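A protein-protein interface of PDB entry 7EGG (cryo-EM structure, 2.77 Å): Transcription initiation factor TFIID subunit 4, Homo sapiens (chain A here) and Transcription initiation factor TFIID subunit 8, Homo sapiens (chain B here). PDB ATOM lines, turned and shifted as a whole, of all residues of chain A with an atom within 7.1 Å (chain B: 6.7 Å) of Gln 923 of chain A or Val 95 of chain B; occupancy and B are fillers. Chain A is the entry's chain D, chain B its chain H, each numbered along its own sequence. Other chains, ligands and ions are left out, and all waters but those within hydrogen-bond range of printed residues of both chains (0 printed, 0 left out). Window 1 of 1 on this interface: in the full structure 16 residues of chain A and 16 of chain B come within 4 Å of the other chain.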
ATOM      1  N   ARG A 851     -16.360   7.719  -9.089  1.00  0.00           N
ATOM      2  CA  ARG A 851     -17.060   7.226 -10.270  1.00  0.00           C
ATOM      3  C   ARG A 851     -16.553   7.925 -11.524  1.00  0.00           C
ATOM      4  O   ARG A 851     -16.411   7.302 -12.585  1.00  0.00           O
ATOM      5  CB  ARG A 851     -18.564   7.441 -10.112  1.00  0.00           C
ATOM      6  CG  ARG A 851     -19.386   7.071 -11.330  1.00  0.00           C
ATOM      7  CD  ARG A 851     -20.605   7.965 -11.525  1.00  0.00           C
ATOM      8  NE  ARG A 851     -21.180   8.474 -10.284  1.00  0.00           N
ATOM      9  CZ  ARG A 851     -21.989   7.783  -9.487  1.00  0.00           C
ATOM     10  NH1 ARG A 851     -22.318   6.534  -9.782  1.00  0.00           N
ATOM     11  NH2 ARG A 851     -22.462   8.344  -8.386  1.00  0.00           N
ATOM     12  N   ALA A 854     -13.414   6.563 -12.534  1.00  0.00           N
ATOM     13  CA  ALA A 854     -13.615   5.242 -13.120  1.00  0.00           C
ATOM     14  C   ALA A 854     -14.067   5.353 -14.571  1.00  0.00           C
ATOM     15  O   ALA A 854     -13.731   4.500 -15.401  1.00  0.00           O
ATOM     16  CB  ALA A 854     -14.626   4.444 -12.296  1.00  0.00           C
ATOM     17  N   GLU A 858     -12.078   4.483 -18.135  1.00  0.00           N
ATOM     18  CA  GLU A 858     -12.841   3.679 -19.099  1.00  0.00           C
ATOM     19  C   GLU A 858     -13.202   2.282 -18.600  1.00  0.00           C
ATOM     20  O   GLU A 858     -14.084   1.628 -19.154  1.00  0.00           O
ATOM     21  CB  GLU A 858     -12.078   3.574 -20.425  1.00  0.00           C
ATOM     22  CG  GLU A 858     -11.966   4.890 -21.176  1.00  0.00           C
ATOM     23  CD  GLU A 858     -10.639   5.584 -20.939  1.00  0.00           C
ATOM     24  OE1 GLU A 858      -9.704   4.927 -20.438  1.00  0.00           O
ATOM     25  OE2 GLU A 858     -10.534   6.788 -21.251  1.00  0.00           O
ATOM     26  N   ILE A 917     -25.250   5.614 -15.328  1.00  0.00           N
ATOM     27  CA  ILE A 917     -25.417   4.588 -16.354  1.00  0.00           C
ATOM     28  C   ILE A 917     -24.208   4.497 -17.272  1.00  0.00           C
ATOM     29  O   ILE A 917     -24.068   3.502 -17.988  1.00  0.00           O
ATOM     30  CB  ILE A 917     -26.678   4.800 -17.208  1.00  0.00           C
ATOM     31  CG1 ILE A 917     -26.554   6.061 -18.065  1.00  0.00           C
ATOM     32  CG2 ILE A 917     -27.928   4.823 -16.340  1.00  0.00           C
ATOM     33  CD1 ILE A 917     -27.762   6.332 -18.919  1.00  0.00           C
ATOM     34  N   SER A 918     -23.328   5.502 -17.276  1.00  0.00           N
ATOM     35  CA  SER A 918     -22.113   5.419 -18.075  1.00  0.00           C
ATOM     36  C   SER A 918     -21.055   4.537 -17.432  1.00  0.00           C
ATOM     37  O   SER A 918     -20.266   3.917 -18.150  1.00  0.00           O
ATOM     38  CB  SER A 918     -21.537   6.813 -18.315  1.00  0.00           C
ATOM     39  OG  SER A 918     -22.273   7.501 -19.306  1.00  0.00           O
ATOM     40  N   GLU A 919     -21.020   4.458 -16.102  1.00  0.00           N
ATOM     41  CA  GLU A 919     -20.051   3.598 -15.437  1.00  0.00           C
ATOM     42  C   GLU A 919     -20.502   2.147 -15.378  1.00  0.00           C
ATOM     43  O   GLU A 919     -19.718   1.288 -14.965  1.00  0.00           O
ATOM     44  CB  GLU A 919     -19.755   4.131 -14.033  1.00  0.00           C
ATOM     45  CG  GLU A 919     -20.963   4.271 -13.123  1.00  0.00           C
ATOM     46  CD  GLU A 919     -21.196   3.055 -12.254  1.00  0.00           C
ATOM     47  OE1 GLU A 919     -20.243   2.279 -12.059  1.00  0.00           O
ATOM     48  OE2 GLU A 919     -22.329   2.879 -11.761  1.00  0.00           O
ATOM     49  N   THR A 920     -21.738   1.853 -15.780  1.00  0.00           N
ATOM     50  CA  THR A 920     -22.164   0.476 -15.967  1.00  0.00           C
ATOM     51  C   THR A 920     -22.310   0.101 -17.435  1.00  0.00           C
ATOM     52  O   THR A 920     -22.407  -1.091 -17.746  1.00  0.00           O
ATOM     53  CB  THR A 920     -23.484   0.208 -15.231  1.00  0.00           C
ATOM     54  OG1 THR A 920     -23.783  -1.190 -15.283  1.00  0.00           O
ATOM     55  CG2 THR A 920     -24.620   0.972 -15.858  1.00  0.00           C
ATOM     56  N   ALA A 921     -22.326   1.082 -18.342  1.00  0.00           N
ATOM     57  CA  ALA A 921     -22.232   0.784 -19.763  1.00  0.00           C
ATOM     58  C   ALA A 921     -20.795   0.566 -20.207  1.00  0.00           C
ATOM     59  O   ALA A 921     -20.572  -0.005 -21.278  1.00  0.00           O
ATOM     60  CB  ALA A 921     -22.855   1.904 -20.594  1.00  0.00           C
ATOM     61  N   GLN A 922     -19.826   1.021 -19.422  1.00  0.00           N
ATOM     62  CA  GLN A 922     -18.425   0.702 -19.646  1.00  0.00           C
ATOM     63  C   GLN A 922     -17.968  -0.488 -18.818  1.00  0.00           C
ATOM     64  O   GLN A 922     -16.818  -0.916 -18.951  1.00  0.00           O
ATOM     65  CB  GLN A 922     -17.551   1.919 -19.339  1.00  0.00           C
ATOM     66  CG  GLN A 922     -17.790   3.084 -20.279  1.00  0.00           C
ATOM     67  CD  GLN A 922     -17.081   4.342 -19.836  1.00  0.00           C
ATOM     68  OE1 GLN A 922     -16.180   4.299 -19.003  1.00  0.00           O
ATOM     69  NE2 GLN A 922     -17.493   5.475 -20.390  1.00  0.00           N
ATOM     70  N   GLN A 923     -18.844  -1.022 -17.965  1.00  0.00           N
ATOM     71  CA  GLN A 923     -18.531  -2.242 -17.233  1.00  0.00           C
ATOM     72  C   GLN A 923     -18.539  -3.455 -18.151  1.00  0.00           C
ATOM     73  O   GLN A 923     -17.838  -4.438 -17.888  1.00  0.00           O
ATOM     74  CB  GLN A 923     -19.531  -2.427 -16.090  1.00  0.00           C
ATOM     75  CG  GLN A 923     -19.063  -3.346 -14.979  1.00  0.00           C
ATOM     76  CD  GLN A 923     -17.966  -2.732 -14.140  1.00  0.00           C
ATOM     77  OE1 GLN A 923     -17.848  -1.511 -14.050  1.00  0.00           O
ATOM     78  NE2 GLN A 923     -17.153  -3.577 -13.520  1.00  0.00           N
ATOM     79  N   LYS A 924     -19.316  -3.402 -19.232  1.00  0.00           N
ATOM     80  CA  LYS A 924     -19.391  -4.488 -20.196  1.00  0.00           C
ATOM     81  C   LYS A 924     -18.316  -4.406 -21.269  1.00  0.00           C
ATOM     82  O   LYS A 924     -18.091  -5.396 -21.971  1.00  0.00           O
ATOM     83  CB  LYS A 924     -20.770  -4.506 -20.863  1.00  0.00           C
ATOM     84  CG  LYS A 924     -21.065  -3.279 -21.713  1.00  0.00           C
ATOM     85  CD  LYS A 924     -22.422  -3.383 -22.394  1.00  0.00           C
ATOM     86  CE  LYS A 924     -22.605  -2.296 -23.443  1.00  0.00           C
ATOM     87  NZ  LYS A 924     -22.804  -0.951 -22.839  1.00  0.00           N
ATOM     88  N   ASN A 925     -17.648  -3.260 -21.413  1.00  0.00           N
ATOM     89  CA  ASN A 925     -16.605  -3.084 -22.415  1.00  0.00           C
ATOM     90  C   ASN A 925     -15.209  -3.310 -21.847  1.00  0.00           C
ATOM     91  O   ASN A 925     -14.234  -2.749 -22.358  1.00  0.00           O
ATOM     92  CB  ASN A 925     -16.701  -1.696 -23.048  1.00  0.00           C
ATOM     93  CG  ASN A 925     -17.965  -1.517 -23.862  1.00  0.00           C
ATOM     94  OD1 ASN A 925     -18.817  -0.693 -23.536  1.00  0.00           O
ATOM     95  ND2 ASN A 925     -18.094  -2.296 -24.929  1.00  0.00           N
ATOM     96  N   PHE A 926     -15.093  -4.118 -20.800  1.00  0.00           N
ATOM     97  CA  PHE A 926     -13.797  -4.509 -20.254  1.00  0.00           C
ATOM     98  C   PHE A 926     -13.526  -5.943 -20.691  1.00  0.00           C
ATOM     99  O   PHE A 926     -14.043  -6.892 -20.098  1.00  0.00           O
ATOM    100  CB  PHE A 926     -13.774  -4.373 -18.737  1.00  0.00           C
ATOM    101  CG  PHE A 926     -12.441  -4.684 -18.125  1.00  0.00           C
ATOM    102  CD1 PHE A 926     -11.384  -3.796 -18.250  1.00  0.00           C
ATOM    103  CD2 PHE A 926     -12.241  -5.865 -17.432  1.00  0.00           C
ATOM    104  CE1 PHE A 926     -10.153  -4.079 -17.689  1.00  0.00           C
ATOM    105  CE2 PHE A 926     -11.011  -6.154 -16.871  1.00  0.00           C
ATOM    106  CZ  PHE A 926      -9.968  -5.259 -17.001  1.00  0.00           C
ATOM    107  N   SER A 927     -12.717  -6.097 -21.735  1.00  0.00           N
ATOM    108  CA  SER A 927     -12.366  -7.418 -22.237  1.00  0.00           C
ATOM    109  C   SER A 927     -11.223  -7.985 -21.408  1.00  0.00           C
ATOM    110  O   SER A 927     -10.121  -7.428 -21.393  1.00  0.00           O
ATOM    111  CB  SER A 927     -11.982  -7.348 -23.713  1.00  0.00           C
ATOM    112  N   TYR A 928     -11.487  -9.094 -20.717  1.00  0.00           N
ATOM    113  CA  TYR A 928     -10.459  -9.728 -19.902  1.00  0.00           C
ATOM    114  C   TYR A 928      -9.465 -10.515 -20.744  1.00  0.00           C
ATOM    115  O   TYR A 928      -8.312 -10.679 -20.334  1.00  0.00           O
ATOM    116  CB  TYR A 928     -11.087 -10.672 -18.877  1.00  0.00           C
ATOM    117  CG  TYR A 928     -11.978 -10.036 -17.837  1.00  0.00           C
ATOM    118  CD1 TYR A 928     -13.313  -9.770 -18.103  1.00  0.00           C
ATOM    119  CD2 TYR A 928     -11.491  -9.740 -16.572  1.00  0.00           C
ATOM    120  CE1 TYR A 928     -14.131  -9.200 -17.149  1.00  0.00           C
ATOM    121  CE2 TYR A 928     -12.302  -9.173 -15.609  1.00  0.00           C
ATOM    122  CZ  TYR A 928     -13.620  -8.906 -15.905  1.00  0.00           C
ATOM    123  OH  TYR A 928     -14.431  -8.341 -14.951  1.00  0.00           O
ATOM    124  N   THR A1056     -19.239   3.316 -27.110  1.00  0.00           N
ATOM    125  CA  THR A1056     -19.957   2.707 -26.000  1.00  0.00           C
ATOM    126  C   THR A1056     -21.439   3.033 -26.112  1.00  0.00           C
ATOM    127  O   THR A1056     -21.821   4.203 -26.196  1.00  0.00           O
ATOM    128  CB  THR A1056     -19.403   3.208 -24.669  1.00  0.00           C
ATOM    129  OG1 THR A1056     -17.999   2.940 -24.604  1.00  0.00           O
ATOM    130  CG2 THR A1056     -20.092   2.508 -23.513  1.00  0.00           C
ATOM    131  N   PHE A1065     -30.679  -1.073 -14.483  1.00  0.00           N
ATOM    132  CA  PHE A1065     -29.736  -1.427 -13.425  1.00  0.00           C
ATOM    133  C   PHE A1065     -29.460  -0.258 -12.490  1.00  0.00           C
ATOM    134  O   PHE A1065     -29.176  -0.465 -11.305  1.00  0.00           O
ATOM    135  CB  PHE A1065     -28.433  -1.923 -14.051  1.00  0.00           C
ATOM    136  CG  PHE A1065     -27.405  -2.355 -13.057  1.00  0.00           C
ATOM    137  CD1 PHE A1065     -27.590  -3.500 -12.307  1.00  0.00           C
ATOM    138  CD2 PHE A1065     -26.242  -1.624 -12.885  1.00  0.00           C
ATOM    139  CE1 PHE A1065     -26.644  -3.900 -11.397  1.00  0.00           C
ATOM    140  CE2 PHE A1065     -25.292  -2.022 -11.975  1.00  0.00           C
ATOM    141  CZ  PHE A1065     -25.492  -3.162 -11.232  1.00  0.00           C
ATOM    142  N   SER B  75     -24.389  -6.294  -4.332  1.00  0.00           N
ATOM    143  CA  SER B  75     -24.093  -5.337  -5.390  1.00  0.00           C
ATOM    144  C   SER B  75     -22.979  -5.799  -6.319  1.00  0.00           C
ATOM    145  O   SER B  75     -22.999  -5.471  -7.508  1.00  0.00           O
ATOM    146  CB  SER B  75     -23.733  -3.979  -4.790  1.00  0.00           C
ATOM    147  OG  SER B  75     -23.820  -2.955  -5.762  1.00  0.00           O
ATOM    148  N   TYR B  79     -23.356  -6.428 -10.268  1.00  0.00           N
ATOM    149  CA  TYR B  79     -22.505  -5.827 -11.287  1.00  0.00           C
ATOM    150  C   TYR B  79     -21.899  -6.875 -12.210  1.00  0.00           C
ATOM    151  O   TYR B  79     -21.667  -6.593 -13.389  1.00  0.00           O
ATOM    152  CB  TYR B  79     -21.405  -4.998 -10.632  1.00  0.00           C
ATOM    153  CG  TYR B  79     -21.721  -3.526 -10.575  1.00  0.00           C
ATOM    154  CD1 TYR B  79     -21.533  -2.716 -11.686  1.00  0.00           C
ATOM    155  CD2 TYR B  79     -22.214  -2.946  -9.413  1.00  0.00           C
ATOM    156  CE1 TYR B  79     -21.823  -1.366 -11.643  1.00  0.00           C
ATOM    157  CE2 TYR B  79     -22.508  -1.595  -9.359  1.00  0.00           C
ATOM    158  CZ  TYR B  79     -22.309  -0.812 -10.479  1.00  0.00           C
ATOM    159  OH  TYR B  79     -22.599   0.530 -10.442  1.00  0.00           O
ATOM    160  N   CYS B  80     -21.633  -8.078 -11.703  1.00  0.00           N
ATOM    161  CA  CYS B  80     -21.094  -9.119 -12.570  1.00  0.00           C
ATOM    162  C   CYS B  80     -22.186  -9.745 -13.426  1.00  0.00           C
ATOM    163  O   CYS B  80     -21.967 -10.009 -14.612  1.00  0.00           O
ATOM    164  CB  CYS B  80     -20.373 -10.185 -11.747  1.00  0.00           C
ATOM    165  SG  CYS B  80     -21.433 -11.314 -10.833  1.00  0.00           S
ATOM    166  N   HIS B  82     -24.845  -8.280 -14.426  1.00  0.00           N
ATOM    167  CA  HIS B  82     -25.167  -7.326 -15.477  1.00  0.00           C
ATOM    168  C   HIS B  82     -24.256  -7.509 -16.680  1.00  0.00           C
ATOM    169  O   HIS B  82     -24.671  -7.265 -17.817  1.00  0.00           O
ATOM    170  CB  HIS B  82     -25.060  -5.903 -14.937  1.00  0.00           C
ATOM    171  CG  HIS B  82     -25.462  -4.853 -15.920  1.00  0.00           C
ATOM    172  ND1 HIS B  82     -26.762  -4.697 -16.350  1.00  0.00           N
ATOM    173  CD2 HIS B  82     -24.737  -3.907 -16.562  1.00  0.00           C
ATOM    174  CE1 HIS B  82     -26.821  -3.701 -17.211  1.00  0.00           C
ATOM    175  NE2 HIS B  82     -25.606  -3.203 -17.357  1.00  0.00           N
ATOM    176  N   THR B  83     -23.018  -7.944 -16.450  1.00  0.00           N
ATOM    177  CA  THR B  83     -22.067  -8.256 -17.509  1.00  0.00           C
ATOM    178  C   THR B  83     -22.075  -9.732 -17.879  1.00  0.00           C
ATOM    179  O   THR B  83     -21.039 -10.260 -18.308  1.00  0.00           O
ATOM    180  CB  THR B  83     -20.665  -7.818 -17.093  1.00  0.00           C
ATOM    181  OG1 THR B  83     -20.250  -8.585 -15.959  1.00  0.00           O
ATOM    182  CG2 THR B  83     -20.664  -6.349 -16.718  1.00  0.00           C
ATOM    183  N   ARG B  85     -21.982 -12.522 -16.317  1.00  0.00           N
ATOM    184  CA  ARG B  85     -21.134 -13.477 -15.617  1.00  0.00           C
ATOM    185  C   ARG B  85     -21.826 -13.966 -14.350  1.00  0.00           C
ATOM    186  O   ARG B  85     -22.868 -13.451 -13.947  1.00  0.00           O
ATOM    187  CB  ARG B  85     -19.775 -12.852 -15.287  1.00  0.00           C
ATOM    188  CG  ARG B  85     -18.878 -12.687 -16.495  1.00  0.00           C
ATOM    189  CD  ARG B  85     -17.539 -12.085 -16.135  1.00  0.00           C
ATOM    190  NE  ARG B  85     -17.598 -10.633 -16.044  1.00  0.00           N
ATOM    191  CZ  ARG B  85     -17.612  -9.960 -14.900  1.00  0.00           C
ATOM    192  NH1 ARG B  85     -17.577 -10.608 -13.746  1.00  0.00           N
ATOM    193  NH2 ARG B  85     -17.665  -8.637 -14.909  1.00  0.00           N
ATOM    194  N   THR B  89     -15.220 -10.835 -10.312  1.00  0.00           N
ATOM    195  CA  THR B  89     -13.782 -10.645 -10.370  1.00  0.00           C
ATOM    196  C   THR B  89     -13.383  -9.473  -9.478  1.00  0.00           C
ATOM    197  O   THR B  89     -14.167  -8.987  -8.659  1.00  0.00           O
ATOM    198  CB  THR B  89     -13.337 -10.419 -11.811  1.00  0.00           C
ATOM    199  OG1 THR B  89     -13.965  -9.238 -12.322  1.00  0.00           O
ATOM    200  CG2 THR B  89     -13.730 -11.594 -12.676  1.00  0.00           C
ATOM    201  N   LEU B  90     -12.142  -9.007  -9.630  1.00  0.00           N
ATOM    202  CA  LEU B  90     -11.699  -7.830  -8.897  1.00  0.00           C
ATOM    203  C   LEU B  90     -12.311  -6.557  -9.463  1.00  0.00           C
ATOM    204  O   LEU B  90     -12.611  -5.626  -8.708  1.00  0.00           O
ATOM    205  CB  LEU B  90     -10.174  -7.748  -8.920  1.00  0.00           C
ATOM    206  CG  LEU B  90      -9.513  -6.592  -8.172  1.00  0.00           C
ATOM    207  CD1 LEU B  90      -9.991  -6.542  -6.736  1.00  0.00           C
ATOM    208  CD2 LEU B  90      -8.016  -6.738  -8.226  1.00  0.00           C
ATOM    209  N   SER B  91     -12.536  -6.508 -10.779  1.00  0.00           N
ATOM    210  CA  SER B  91     -13.068  -5.310 -11.415  1.00  0.00           C
ATOM    211  C   SER B  91     -14.537  -5.071 -11.090  1.00  0.00           C
ATOM    212  O   SER B  91     -15.045  -3.976 -11.354  1.00  0.00           O
ATOM    213  CB  SER B  91     -12.885  -5.395 -12.931  1.00  0.00           C
ATOM    214  OG  SER B  91     -11.512  -5.432 -13.276  1.00  0.00           O
ATOM    215  N   ASP B  92     -15.228  -6.061 -10.530  1.00  0.00           N
ATOM    216  CA  ASP B  92     -16.612  -5.904 -10.114  1.00  0.00           C
ATOM    217  C   ASP B  92     -16.747  -5.406  -8.686  1.00  0.00           C
ATOM    218  O   ASP B  92     -17.824  -4.935  -8.315  1.00  0.00           O
ATOM    219  CB  ASP B  92     -17.359  -7.232 -10.247  1.00  0.00           C
ATOM    220  CG  ASP B  92     -17.565  -7.639 -11.685  1.00  0.00           C
ATOM    221  OD1 ASP B  92     -17.949  -6.779 -12.504  1.00  0.00           O
ATOM    222  OD2 ASP B  92     -17.338  -8.824 -12.000  1.00  0.00           O
ATOM    223  N   ILE B  93     -15.690  -5.499  -7.882  1.00  0.00           N
ATOM    224  CA  ILE B  93     -15.737  -5.079  -6.487  1.00  0.00           C
ATOM    225  C   ILE B  93     -15.161  -3.677  -6.373  1.00  0.00           C
ATOM    226  O   ILE B  93     -15.644  -2.856  -5.585  1.00  0.00           O
ATOM    227  CB  ILE B  93     -14.992  -6.079  -5.587  1.00  0.00           C
ATOM    228  CG1 ILE B  93     -15.513  -7.487  -5.861  1.00  0.00           C
ATOM    229  CG2 ILE B  93     -15.171  -5.726  -4.119  1.00  0.00           C
ATOM    230  CD1 ILE B  93     -15.012  -8.524  -4.908  1.00  0.00           C
ATOM    231  N   VAL B  94     -14.152  -3.366  -7.194  1.00  0.00           N
ATOM    232  CA  VAL B  94     -13.616  -2.006  -7.221  1.00  0.00           C
ATOM    233  C   VAL B  94     -14.545  -1.028  -7.915  1.00  0.00           C
ATOM    234  O   VAL B  94     -14.299   0.181  -7.857  1.00  0.00           O
ATOM    235  CB  VAL B  94     -12.231  -1.940  -7.893  1.00  0.00           C
ATOM    236  CG1 VAL B  94     -11.279  -2.923  -7.239  1.00  0.00           C
ATOM    237  CG2 VAL B  94     -12.342  -2.196  -9.383  1.00  0.00           C
ATOM    238  N   VAL B  95     -15.591  -1.506  -8.585  1.00  0.00           N
ATOM    239  CA  VAL B  95     -16.695  -0.646  -8.986  1.00  0.00           C
ATOM    240  C   VAL B  95     -17.827  -0.692  -7.961  1.00  0.00           C
ATOM    241  O   VAL B  95     -18.569   0.292  -7.829  1.00  0.00           O
ATOM    242  CB  VAL B  95     -17.192  -0.997 -10.411  1.00  0.00           C
ATOM    243  CG1 VAL B  95     -18.000  -2.289 -10.456  1.00  0.00           C
ATOM    244  CG2 VAL B  95     -17.961   0.155 -11.024  1.00  0.00           C
ATOM    245  N   THR B  96     -17.965  -1.791  -7.214  1.00  0.00           N
ATOM    246  CA  THR B  96     -18.934  -1.881  -6.130  1.00  0.00           C
ATOM    247  C   THR B  96     -18.548  -0.989  -4.959  1.00  0.00           C
ATOM    248  O   THR B  96     -19.402  -0.311  -4.379  1.00  0.00           O
ATOM    249  CB  THR B  96     -19.049  -3.333  -5.680  1.00  0.00           C
ATOM    250  OG1 THR B  96     -19.395  -4.141  -6.806  1.00  0.00           O
ATOM    251  CG2 THR B  96     -20.097  -3.497  -4.611  1.00  0.00           C
ATOM    252  N   LEU B  97     -17.261  -0.966  -4.613  1.00  0.00           N
ATOM    253  CA  LEU B  97     -16.809  -0.150  -3.496  1.00  0.00           C
ATOM    254  C   LEU B  97     -16.776   1.327  -3.862  1.00  0.00           C
ATOM    255  O   LEU B  97     -16.916   2.182  -2.982  1.00  0.00           O
ATOM    256  CB  LEU B  97     -15.435  -0.623  -3.034  1.00  0.00           C
ATOM    257  CG  LEU B  97     -15.398  -1.984  -2.345  1.00  0.00           C
ATOM    258  CD1 LEU B  97     -13.968  -2.393  -2.064  1.00  0.00           C
ATOM    259  CD2 LEU B  97     -16.198  -1.941  -1.067  1.00  0.00           C
ATOM    260  N   VAL B  98     -16.579   1.642  -5.144  1.00  0.00           N
ATOM    261  CA  VAL B  98     -16.693   3.023  -5.611  1.00  0.00           C
ATOM    262  C   VAL B  98     -18.125   3.519  -5.461  1.00  0.00           C
ATOM    263  O   VAL B  98     -18.362   4.641  -4.992  1.00  0.00           O
ATOM    264  CB  VAL B  98     -16.177   3.131  -7.060  1.00  0.00           C
ATOM    265  CG1 VAL B  98     -16.828   4.280  -7.813  1.00  0.00           C
ATOM    266  CG2 VAL B  98     -14.677   3.326  -7.047  1.00  0.00           C
ATOM    267  N   GLU B  99     -19.105   2.674  -5.787  1.00  0.00           N
ATOM    268  CA  GLU B  99     -20.503   3.066  -5.648  1.00  0.00           C
ATOM    269  C   GLU B  99     -20.981   3.092  -4.200  1.00  0.00           C
ATOM    270  O   GLU B  99     -22.124   3.490  -3.958  1.00  0.00           O
ATOM    271  CB  GLU B  99     -21.402   2.139  -6.467  1.00  0.00           C
ATOM    272  CG  GLU B  99     -21.190   2.236  -7.969  1.00  0.00           C
ATOM    273  CD  GLU B  99     -21.137   3.665  -8.475  1.00  0.00           C
ATOM    274  OE1 GLU B  99     -22.111   4.416  -8.260  1.00  0.00           O
ATOM    275  OE2 GLU B  99     -20.120   4.037  -9.094  1.00  0.00           O
ATOM    276  N   MET B 100     -20.149   2.691  -3.245  1.00  0.00           N
ATOM    277  CA  MET B 100     -20.415   2.907  -1.832  1.00  0.00           C
ATOM    278  C   MET B 100     -19.531   3.984  -1.229  1.00  0.00           C
ATOM    279  O   MET B 100     -19.624   4.230  -0.025  1.00  0.00           O
ATOM    280  CB  MET B 100     -20.230   1.611  -1.044  1.00  0.00           C
ATOM    281  CG  MET B 100     -21.285   0.574  -1.301  1.00  0.00           C
ATOM    282  SD  MET B 100     -21.033  -0.884  -0.284  1.00  0.00           S
ATOM    283  CE  MET B 100     -21.533  -2.137  -1.445  1.00  0.00           C
ATOM    284  N   VAL B 104     -10.790   3.108  -2.475  1.00  0.00           N
ATOM    285  CA  VAL B 104     -10.163   1.786  -2.445  1.00  0.00           C
ATOM    286  C   VAL B 104      -8.639   1.829  -2.291  1.00  0.00           C
ATOM    287  O   VAL B 104      -8.058   0.922  -1.684  1.00  0.00           O
ATOM    288  CB  VAL B 104     -10.610   1.053  -3.739  1.00  0.00           C
ATOM    289  CG1 VAL B 104      -9.890  -0.276  -3.972  1.00  0.00           C
ATOM    290  CG2 VAL B 104     -12.113   0.853  -3.730  1.00  0.00           C
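NH1 of Arg 851 of chain A lies within salt-bridge range of OE1 of Glu 99 of chain B (2.6 Å). The side-chain carboxylate (OE2) of Glu 919 of chain A lies within hydrogen-bond range of the side-chain hydroxyl (OH) of Tyr 79 of chain B. OG1 of Thr 920 of chain A lies close to NE2 of His 82 of chain B (3.4 Å). The backbone carbonyl oxygen of Ser 91 of chain B sits at hydrogen-bond distance from the side-chain amide nitrogen of Gln 923 of chain A. The side-chain amide nitrogen (NE2) of Gln 923 of chain A is in hydrogen-bond range of the side-chain carboxylate (OD1) of Asp 92 of chain B (3.5 Å). OH of Tyr 928 of chain A is in hydrogen-bond range of NH2 of Arg 85 of chain B. The side-chain hydroxyl of Thr 89 of chain B is in hydrogen-bond range of the side-chain hydroxyl of Tyr 928 of chain A (2.8 Å). The side-chain carboxylate of Glu 919 of chain A sits close to the side-chain carboxylate of Glu 99 of chain B (3.4 Å).
The backbone carbonyl oxygen (O) of Glu 919 of chain A sits close to the side-chain amide oxygen (OE1) of Gln 923 of chain A (3.5 Å). The side-chain hydroxyl (OG1) of Thr 83 of chain B lies within hydrogen-bond range of the backbone carbonyl oxygen (O) of Cys 80 of chain B. The side-chain hydroxyl (OG1) of Thr 83 of chain B lies within hydrogen-bond range of the guanidinium group (NH2) of Arg 85 of chain B (2.8 Å). OD2 of Asp 92 of chain B is in salt-bridge range of NH1 of Arg 85 of chain B (2.5 Å). N of Ser 91 of chain B lies close to OG1 of Thr 89 of chain B. The backbone NH of Thr 89 of chain B sits at hydrogen-bond distance from the side-chain carboxylate of Asp 92 of chain B, 3.4 Å away.
N of Arg 851 of chain A touches CG1 of Val 98 of chain B, at 3.7 Å. Val 95 of chain B touches Glu 919 of chain A (CG2 to OE1, 3.3 Å). Gln 923 of chain A touches Thr 83 of chain B (O to CG2, 3.6 Å). Val 95 of chain B touches Gln 923 of chain A (CG1 to NE2, 3.4 Å). Ser 91 of chain B touches Phe 926 of chain A. Tyr 928 of chain A touches Ser 91 of chain B (OH to CB, 3.9 Å). Tyr 79 of chain B touches Phe 1065 of chain A (CE1 to CE2, 3.5 Å). His 82 of chain B touches Phe 1065 of chain A.
Printed residues of chain B within 4 Å of Arg 851 of chain A: Val 98 (3.7 Å) and Glu 99 (2.6 Å). Gln 923 of chain A touches just these residues of chain B: Thr 83 (3.6 Å), Ser 91 (3.0 Å), Asp 92 (3.5 Å) and Val 95 (3.4 Å). Printed residues of chain A within 4 Å of Tyr 79 of chain B: Glu 919 (2.7 Å) and Phe 1065 (3.5 Å). Printed residues of chain A within 4 Å of His 82 of chain B: Thr 920 (3.2 Å) and Phe 1065 (3.97 Å). Of the printed residues of chain A, Arg 85 of chain B touches Tyr 928. Val 95 of chain B touches just these residues of chain A: Glu 919 (3.3 Å) and Gln 923 (3.4 Å). Printed residues of chain A within 4 Å of Val 98 of chain B: Arg 851 (3.7 Å). The nearest residue of chain B that does not touch Gln 923 of chain A is Tyr 79 of chain B (4.2 Å). The nearest residue of chain A that does not touch Val 95 of chain B is Ala 854 of chain A (5.6 Å).
Along chain B the printed residues that touch a printed residue of chain A span positions 79 to 99. Of the 17 printed residues of chain A, 7 touch a printed residue of chain B. Hydrophobic or aromatic side chains of chain A within 4 Å of the printed part of chain B: Phe 926, Tyr 928 and Phe 1065. Along chain A the printed residues that touch a printed residue of chain B span positions 851 to 1065. Among the printed residues, 16 pairs touch across the chains. Among the printed residues, Asp or Glu carboxylates within 4 Å of a Lys or Arg side-chain nitrogen of the other chain: Arg 851 of chain A with Glu 99 of chain B (2.6 Å).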
